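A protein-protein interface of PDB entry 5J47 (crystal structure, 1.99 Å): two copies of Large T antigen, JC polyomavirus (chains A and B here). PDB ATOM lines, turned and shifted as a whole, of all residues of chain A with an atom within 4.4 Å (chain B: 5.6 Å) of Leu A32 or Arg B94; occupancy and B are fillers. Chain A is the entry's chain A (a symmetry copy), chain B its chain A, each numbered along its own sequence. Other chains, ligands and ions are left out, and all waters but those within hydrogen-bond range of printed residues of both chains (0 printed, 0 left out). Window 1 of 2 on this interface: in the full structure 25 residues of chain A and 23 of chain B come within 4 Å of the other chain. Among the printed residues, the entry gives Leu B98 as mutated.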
ATOM      1  N   ASP A  29     -22.637  -8.114  22.738  1.00  0.00           N
ATOM      2  CA  ASP A  29     -21.285  -8.579  23.062  1.00  0.00           C
ATOM      3  C   ASP A  29     -20.549  -7.471  23.820  1.00  0.00           C
ATOM      4  O   ASP A  29     -20.293  -6.401  23.253  1.00  0.00           O
ATOM      5  CB  ASP A  29     -20.570  -8.937  21.739  1.00  0.00           C
ATOM      6  CG  ASP A  29     -19.268  -9.718  21.819  1.00  0.00           C
ATOM      7  OD1 ASP A  29     -18.559  -9.602  22.852  1.00  0.00           O
ATOM      8  OD2 ASP A  29     -18.921 -10.391  20.818  1.00  0.00           O
ATOM      9  N   VAL A  30     -20.256  -7.718  25.110  1.00  0.00           N
ATOM     10  CA  VAL A  30     -19.590  -6.780  26.030  1.00  0.00           C
ATOM     11  C   VAL A  30     -18.200  -6.377  25.505  1.00  0.00           C
ATOM     12  O   VAL A  30     -17.841  -5.200  25.570  1.00  0.00           O
ATOM     13  CB  VAL A  30     -19.536  -7.332  27.492  1.00  0.00           C
ATOM     14  CG1 VAL A  30     -18.748  -6.415  28.424  1.00  0.00           C
ATOM     15  CG2 VAL A  30     -20.938  -7.563  28.053  1.00  0.00           C
ATOM     16  N   PHE A  31     -17.434  -7.354  24.986  1.00  0.00           N
ATOM     17  CA  PHE A  31     -16.094  -7.123  24.437  1.00  0.00           C
ATOM     18  C   PHE A  31     -16.150  -6.340  23.132  1.00  0.00           C
ATOM     19  O   PHE A  31     -15.362  -5.408  22.953  1.00  0.00           O
ATOM     20  CB  PHE A  31     -15.320  -8.440  24.293  1.00  0.00           C
ATOM     21  CG  PHE A  31     -14.910  -9.009  25.637  1.00  0.00           C
ATOM     22  CD1 PHE A  31     -13.715  -8.627  26.237  1.00  0.00           C
ATOM     23  CD2 PHE A  31     -15.745  -9.885  26.327  1.00  0.00           C
ATOM     24  CE1 PHE A  31     -13.354  -9.124  27.496  1.00  0.00           C
ATOM     25  CE2 PHE A  31     -15.382 -10.382  27.584  1.00  0.00           C
ATOM     26  CZ  PHE A  31     -14.188  -9.998  28.161  1.00  0.00           C
ATOM     27  N   LEU A  32     -17.109  -6.669  22.241  1.00  0.00           N
ATOM     28  CA  LEU A  32     -17.254  -5.931  20.977  1.00  0.00           C
ATOM     29  C   LEU A  32     -17.591  -4.471  21.271  1.00  0.00           C
ATOM     30  O   LEU A  32     -16.959  -3.585  20.703  1.00  0.00           O
ATOM     31  CB  LEU A  32     -18.301  -6.559  20.034  1.00  0.00           C
ATOM     32  CG  LEU A  32     -18.395  -5.963  18.619  1.00  0.00           C
ATOM     33  CD1 LEU A  32     -17.096  -6.175  17.823  1.00  0.00           C
ATOM     34  CD2 LEU A  32     -19.587  -6.534  17.870  1.00  0.00           C
ATOM     35  N   LEU A  33     -18.515  -4.232  22.216  1.00  0.00           N
ATOM     36  CA  LEU A  33     -18.925  -2.888  22.630  1.00  0.00           C
ATOM     37  C   LEU A  33     -17.725  -2.088  23.135  1.00  0.00           C
ATOM     38  O   LEU A  33     -17.527  -0.956  22.706  1.00  0.00           O
ATOM     39  CB  LEU A  33     -20.007  -2.967  23.717  1.00  0.00           C
ATOM     40  CG  LEU A  33     -20.486  -1.638  24.314  1.00  0.00           C
ATOM     41  CD1 LEU A  33     -21.078  -0.733  23.255  1.00  0.00           C
ATOM     42  CD2 LEU A  33     -21.535  -1.879  25.352  1.00  0.00           C
ATOM     43  N   MET A  34     -16.940  -2.679  24.041  1.00  0.00           N
ATOM     44  CA  MET A  34     -15.742  -2.075  24.616  1.00  0.00           C
ATOM     45  C   MET A  34     -14.751  -1.648  23.527  1.00  0.00           C
ATOM     46  O   MET A  34     -14.289  -0.503  23.529  1.00  0.00           O
ATOM     47  CB  MET A  34     -15.100  -3.080  25.579  1.00  0.00           C
ATOM     48  CG  MET A  34     -14.158  -2.462  26.544  1.00  0.00           C
ATOM     49  SD  MET A  34     -13.726  -3.669  27.828  1.00  0.00           S
ATOM     50  CE  MET A  34     -12.107  -3.136  28.165  1.00  0.00           C
ATOM     51  N   GLY A  35     -14.458  -2.559  22.601  1.00  0.00           N
ATOM     52  CA  GLY A  35     -13.544  -2.297  21.492  1.00  0.00           C
ATOM     53  C   GLY A  35     -14.053  -1.220  20.543  1.00  0.00           C
ATOM     54  O   GLY A  35     -13.284  -0.342  20.133  1.00  0.00           O
ATOM     55  N   MET A  36     -15.358  -1.278  20.185  1.00  0.00           N
ATOM     56  CA  MET A  36     -15.982  -0.291  19.293  1.00  0.00           C
ATOM     57  C   MET A  36     -15.982   1.103  19.924  1.00  0.00           C
ATOM     58  O   MET A  36     -15.633   2.071  19.243  1.00  0.00           O
ATOM     59  CB  MET A  36     -17.418  -0.701  18.904  1.00  0.00           C
ATOM     60  CG  MET A  36     -17.491  -1.899  17.961  1.00  0.00           C
ATOM     61  SD  MET A  36     -16.664  -1.678  16.366  1.00  0.00           S
ATOM     62  CE  MET A  36     -17.767  -0.472  15.581  1.00  0.00           C
ATOM     63  N   VAL B  89      -7.362  -5.984  25.037  1.00  0.00           N
ATOM     64  CA  VAL B  89      -6.660  -6.735  23.990  1.00  0.00           C
ATOM     65  C   VAL B  89      -7.671  -7.688  23.332  1.00  0.00           C
ATOM     66  O   VAL B  89      -7.733  -7.734  22.105  1.00  0.00           O
ATOM     67  CB  VAL B  89      -5.367  -7.436  24.506  1.00  0.00           C
ATOM     68  CG1 VAL B  89      -4.743  -8.334  23.438  1.00  0.00           C
ATOM     69  CG2 VAL B  89      -4.347  -6.409  24.974  1.00  0.00           C
ATOM     70  N   ALA B  90      -8.506  -8.383  24.151  1.00  0.00           N
ATOM     71  CA  ALA B  90      -9.565  -9.273  23.656  1.00  0.00           C
ATOM     72  C   ALA B  90     -10.623  -8.478  22.871  1.00  0.00           C
ATOM     73  O   ALA B  90     -11.101  -8.952  21.840  1.00  0.00           O
ATOM     74  CB  ALA B  90     -10.220 -10.009  24.812  1.00  0.00           C
ATOM     75  N   ALA B  91     -10.974  -7.267  23.358  1.00  0.00           N
ATOM     76  CA  ALA B  91     -11.939  -6.352  22.728  1.00  0.00           C
ATOM     77  C   ALA B  91     -11.457  -5.924  21.339  1.00  0.00           C
ATOM     78  O   ALA B  91     -12.236  -5.964  20.392  1.00  0.00           O
ATOM     79  CB  ALA B  91     -12.158  -5.128  23.613  1.00  0.00           C
ATOM     80  N   LYS B  92     -10.167  -5.551  21.218  1.00  0.00           N
ATOM     81  CA  LYS B  92      -9.525  -5.166  19.961  1.00  0.00           C
ATOM     82  C   LYS B  92      -9.571  -6.360  18.993  1.00  0.00           C
ATOM     83  O   LYS B  92      -9.884  -6.176  17.821  1.00  0.00           O
ATOM     84  CB  LYS B  92      -8.055  -4.771  20.226  1.00  0.00           C
ATOM     85  CG  LYS B  92      -7.575  -3.548  19.444  1.00  0.00           C
ATOM     86  CD  LYS B  92      -7.107  -3.875  18.042  1.00  0.00           C
ATOM     87  CE  LYS B  92      -5.607  -3.937  17.932  1.00  0.00           C
ATOM     88  NZ  LYS B  92      -5.172  -4.202  16.536  1.00  0.00           N
ATOM     89  N   GLN B  93      -9.273  -7.585  19.495  1.00  0.00           N
ATOM     90  CA  GLN B  93      -9.329  -8.811  18.687  1.00  0.00           C
ATOM     91  C   GLN B  93     -10.745  -9.065  18.123  1.00  0.00           C
ATOM     92  O   GLN B  93     -10.860  -9.521  16.990  1.00  0.00           O
ATOM     93  CB  GLN B  93      -8.844 -10.021  19.499  1.00  0.00           C
ATOM     94  CG  GLN B  93      -8.106 -11.065  18.659  1.00  0.00           C
ATOM     95  CD  GLN B  93      -6.709 -10.633  18.255  1.00  0.00           C
ATOM     96  OE1 GLN B  93      -6.382 -10.534  17.067  1.00  0.00           O
ATOM     97  NE2 GLN B  93      -5.850 -10.373  19.234  1.00  0.00           N
ATOM     98  N   ARG B  94     -11.813  -8.756  18.905  1.00  0.00           N
ATOM     99  CA  ARG B  94     -13.220  -8.905  18.493  1.00  0.00           C
ATOM    100  C   ARG B  94     -13.545  -7.948  17.345  1.00  0.00           C
ATOM    101  O   ARG B  94     -14.205  -8.340  16.382  1.00  0.00           O
ATOM    102  CB  ARG B  94     -14.182  -8.603  19.666  1.00  0.00           C
ATOM    103  CG  ARG B  94     -14.229  -9.678  20.723  1.00  0.00           C
ATOM    104  CD  ARG B  94     -15.646 -10.152  20.921  1.00  0.00           C
ATOM    105  NE  ARG B  94     -15.699 -11.573  21.260  1.00  0.00           N
ATOM    106  CZ  ARG B  94     -15.678 -12.551  20.361  1.00  0.00           C
ATOM    107  NH1 ARG B  94     -15.593 -12.269  19.065  1.00  0.00           N
ATOM    108  NH2 ARG B  94     -15.729 -13.817  20.749  1.00  0.00           N
ATOM    109  N   VAL B  95     -13.085  -6.690  17.473  1.00  0.00           N
ATOM    110  CA  VAL B  95     -13.252  -5.615  16.493  1.00  0.00           C
ATOM    111  C   VAL B  95     -12.525  -5.990  15.188  1.00  0.00           C
ATOM    112  O   VAL B  95     -13.108  -5.848  14.115  1.00  0.00           O
ATOM    113  CB  VAL B  95     -12.770  -4.257  17.079  1.00  0.00           C
ATOM    114  CG1 VAL B  95     -12.616  -3.182  15.999  1.00  0.00           C
ATOM    115  CG2 VAL B  95     -13.711  -3.779  18.170  1.00  0.00           C
ATOM    116  N   ASP B  96     -11.279  -6.496  15.292  1.00  0.00           N
ATOM    117  CA  ASP B  96     -10.469  -6.887  14.127  1.00  0.00           C
ATOM    118  C   ASP B  96     -11.049  -8.089  13.403  1.00  0.00           C
ATOM    119  O   ASP B  96     -11.105  -8.077  12.175  1.00  0.00           O
ATOM    120  CB  ASP B  96      -9.006  -7.151  14.521  1.00  0.00           C
ATOM    121  CG  ASP B  96      -8.249  -5.944  15.041  1.00  0.00           C
ATOM    122  OD1 ASP B  96      -8.711  -4.797  14.807  1.00  0.00           O
ATOM    123  OD2 ASP B  96      -7.169  -6.138  15.630  1.00  0.00           O
ATOM    124  N   SER B  97     -11.535  -9.100  14.152  1.00  0.00           N
ATOM    125  CA  SER B  97     -12.150 -10.293  13.567  1.00  0.00           C
ATOM    126  C   SER B  97     -13.339  -9.939  12.673  1.00  0.00           C
ATOM    127  O   SER B  97     -13.592 -10.644  11.700  1.00  0.00           O
ATOM    128  CB  SER B  97     -12.558 -11.286  14.651  1.00  0.00           C
ATOM    129  OG  SER B  97     -13.732 -10.861  15.323  1.00  0.00           O
ATOM    130  N   LEU B  98     -14.028  -8.820  12.966  1.00  0.00           N
ATOM    131  CA  LEU B  98     -15.182  -8.357  12.188  1.00  0.00           C
ATOM    132  C   LEU B  98     -14.866  -7.290  11.122  1.00  0.00           C
ATOM    133  O   LEU B  98     -15.578  -7.233  10.117  1.00  0.00           O
ATOM    134  CB  LEU B  98     -16.307  -7.864  13.121  1.00  0.00           C
ATOM    135  CG  LEU B  98     -17.169  -8.957  13.770  1.00  0.00           C
ATOM    136  CD1 LEU B  98     -17.835  -8.454  15.015  1.00  0.00           C
ATOM    137  CD2 LEU B  98     -18.228  -9.482  12.814  1.00  0.00           C
ATOM    138  N   HIS B  99     -13.835  -6.442  11.332  1.00  0.00           N
ATOM    139  CA  HIS B  99     -13.499  -5.340  10.414  1.00  0.00           C
ATOM    140  C   HIS B  99     -12.279  -5.556   9.538  1.00  0.00           C
ATOM    141  O   HIS B  99     -12.226  -5.029   8.423  1.00  0.00           O
ATOM    142  CB  HIS B  99     -13.331  -4.030  11.198  1.00  0.00           C
ATOM    143  N   ILE B 210     -12.440 -19.763  18.143  1.00  0.00           N
ATOM    144  CA  ILE B 210     -13.039 -18.421  18.207  1.00  0.00           C
ATOM    145  C   ILE B 210     -11.977 -17.342  17.924  1.00  0.00           C
ATOM    146  O   ILE B 210     -10.904 -17.367  18.527  1.00  0.00           O
ATOM    147  CB  ILE B 210     -13.828 -18.190  19.533  1.00  0.00           C
ATOM    148  CG1 ILE B 210     -15.042 -19.145  19.618  1.00  0.00           C
ATOM    149  CG2 ILE B 210     -14.289 -16.724  19.677  1.00  0.00           C
ATOM    150  CD1 ILE B 210     -15.665 -19.298  21.006  1.00  0.00           C
ATOM    151  N   ASP B 211     -12.277 -16.431  16.961  1.00  0.00           N
ATOM    152  CA  ASP B 211     -11.420 -15.324  16.501  1.00  0.00           C
ATOM    153  C   ASP B 211     -10.082 -15.782  15.897  1.00  0.00           C
ATOM    154  O   ASP B 211      -9.185 -14.955  15.717  1.00  0.00           O
ATOM    155  CB  ASP B 211     -11.188 -14.270  17.616  1.00  0.00           C
ATOM    156  CG  ASP B 211     -12.435 -13.645  18.218  1.00  0.00           C
ATOM    157  OD1 ASP B 211     -13.384 -13.348  17.454  1.00  0.00           O
ATOM    158  OD2 ASP B 211     -12.428 -13.372  19.439  1.00  0.00           O
ATOM    159  N   LYS B 261     -20.389 -18.255  23.280  1.00  0.00           N
ATOM    160  CA  LYS B 261     -19.375 -17.198  23.272  1.00  0.00           C
ATOM    161  C   LYS B 261     -19.377 -16.369  21.977  1.00  0.00           C
ATOM    162  O   LYS B 261     -19.337 -15.141  22.064  1.00  0.00           O
ATOM    163  CB  LYS B 261     -17.978 -17.769  23.569  1.00  0.00           C
ATOM    164  N   ARG B 262     -19.426 -17.023  20.787  1.00  0.00           N
ATOM    165  CA  ARG B 262     -19.433 -16.321  19.497  1.00  0.00           C
ATOM    166  C   ARG B 262     -20.077 -17.108  18.346  1.00  0.00           C
ATOM    167  O   ARG B 262     -19.905 -18.323  18.241  1.00  0.00           O
ATOM    168  CB  ARG B 262     -18.009 -15.875  19.095  1.00  0.00           C
ATOM    169  CG  ARG B 262     -17.989 -14.628  18.209  1.00  0.00           C
ATOM    170  CD  ARG B 262     -16.834 -14.651  17.230  1.00  0.00           C
ATOM    171  NE  ARG B 262     -16.918 -13.557  16.257  1.00  0.00           N
ATOM    172  CZ  ARG B 262     -16.042 -13.349  15.277  1.00  0.00           C
ATOM    173  NH1 ARG B 262     -14.995 -14.151  15.131  1.00  0.00           N
ATOM    174  NH2 ARG B 262     -16.206 -12.335  14.439  1.00  0.00           N
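The guanidinium group (NE) of Arg B94 lies within salt-bridge range of the side-chain carboxylate (OD2) of Asp A29, at 3.5 Å.
The side-chain carboxylate (OD1) of Asp A29 is in hydrogen-bond range of the backbone NH (N) of Leu A32, 3.3 Å away.
NH1 of Arg B94 lies within salt-bridge range of OD1 of Asp B211 (2.9 Å).
The backbone NH (N) of Phe A31 is in hydrogen-bond range of the side-chain carboxylate (OD1) of Asp A29.
The backbone carbonyl oxygen of Arg B94 is in hydrogen-bond range of the side-chain hydroxyl of Ser B97 (2.8 Å).
Among the printed residues, pairs that only touch across the chains: Phe A31 with Ala B91 (3.3 Å), Phe A31 with Arg B94 (3.8 Å), Leu A32 with Arg B94 (3.9 Å), Leu A32 with Leu B98 (3.7 Å), Gly A35 with Ala B91 (3.6 Å), Gly A35 with Val B95 (3.5 Å) and Met A36 with Val B95 (3.6 Å).
Of the printed residues of chain B, Asp A29 touches Arg B94 (3.3 Å).
Of chain B, only Arg B94 (3.9 Å) and Leu B98 (3.7 Å) come within 4 Å of Leu A32.
Printed residues of chain B within 4 Å of Gly A35: Ala B91 (3.6 Å) and Val B95 (3.5 Å).
Val B89 touches none of the printed residues of chain A.
Arg B94 touches three residues of chain A.
Printed residues of chain A within 4 Å of Leu B98: Leu A32.
Arg B262 touches none of the printed residues of chain A.
The nearest printed residue of chain A that does not touch Arg B94 is Val A30 (6.5 Å).
Hydrophobic or aromatic side chains of chain A that line the printed part of chain B: Phe A31 and Leu A32.
Of the 15 printed residues of chain B, 4 touch a printed residue of chain A.
Printed residues of chain B that touch a printed residue of chain A: Ala B91, Arg B94, Val B95 and Leu B98.
Among the printed residues, Asp or Glu carboxylates within 4 Å of a Lys or Arg side-chain nitrogen of the other chain: Asp A29 with Arg B94.
No position is printed for both chains.
Of the 8 pairs that touch across the chains among the printed residues, none has its exchanged pair printed and touching as well.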
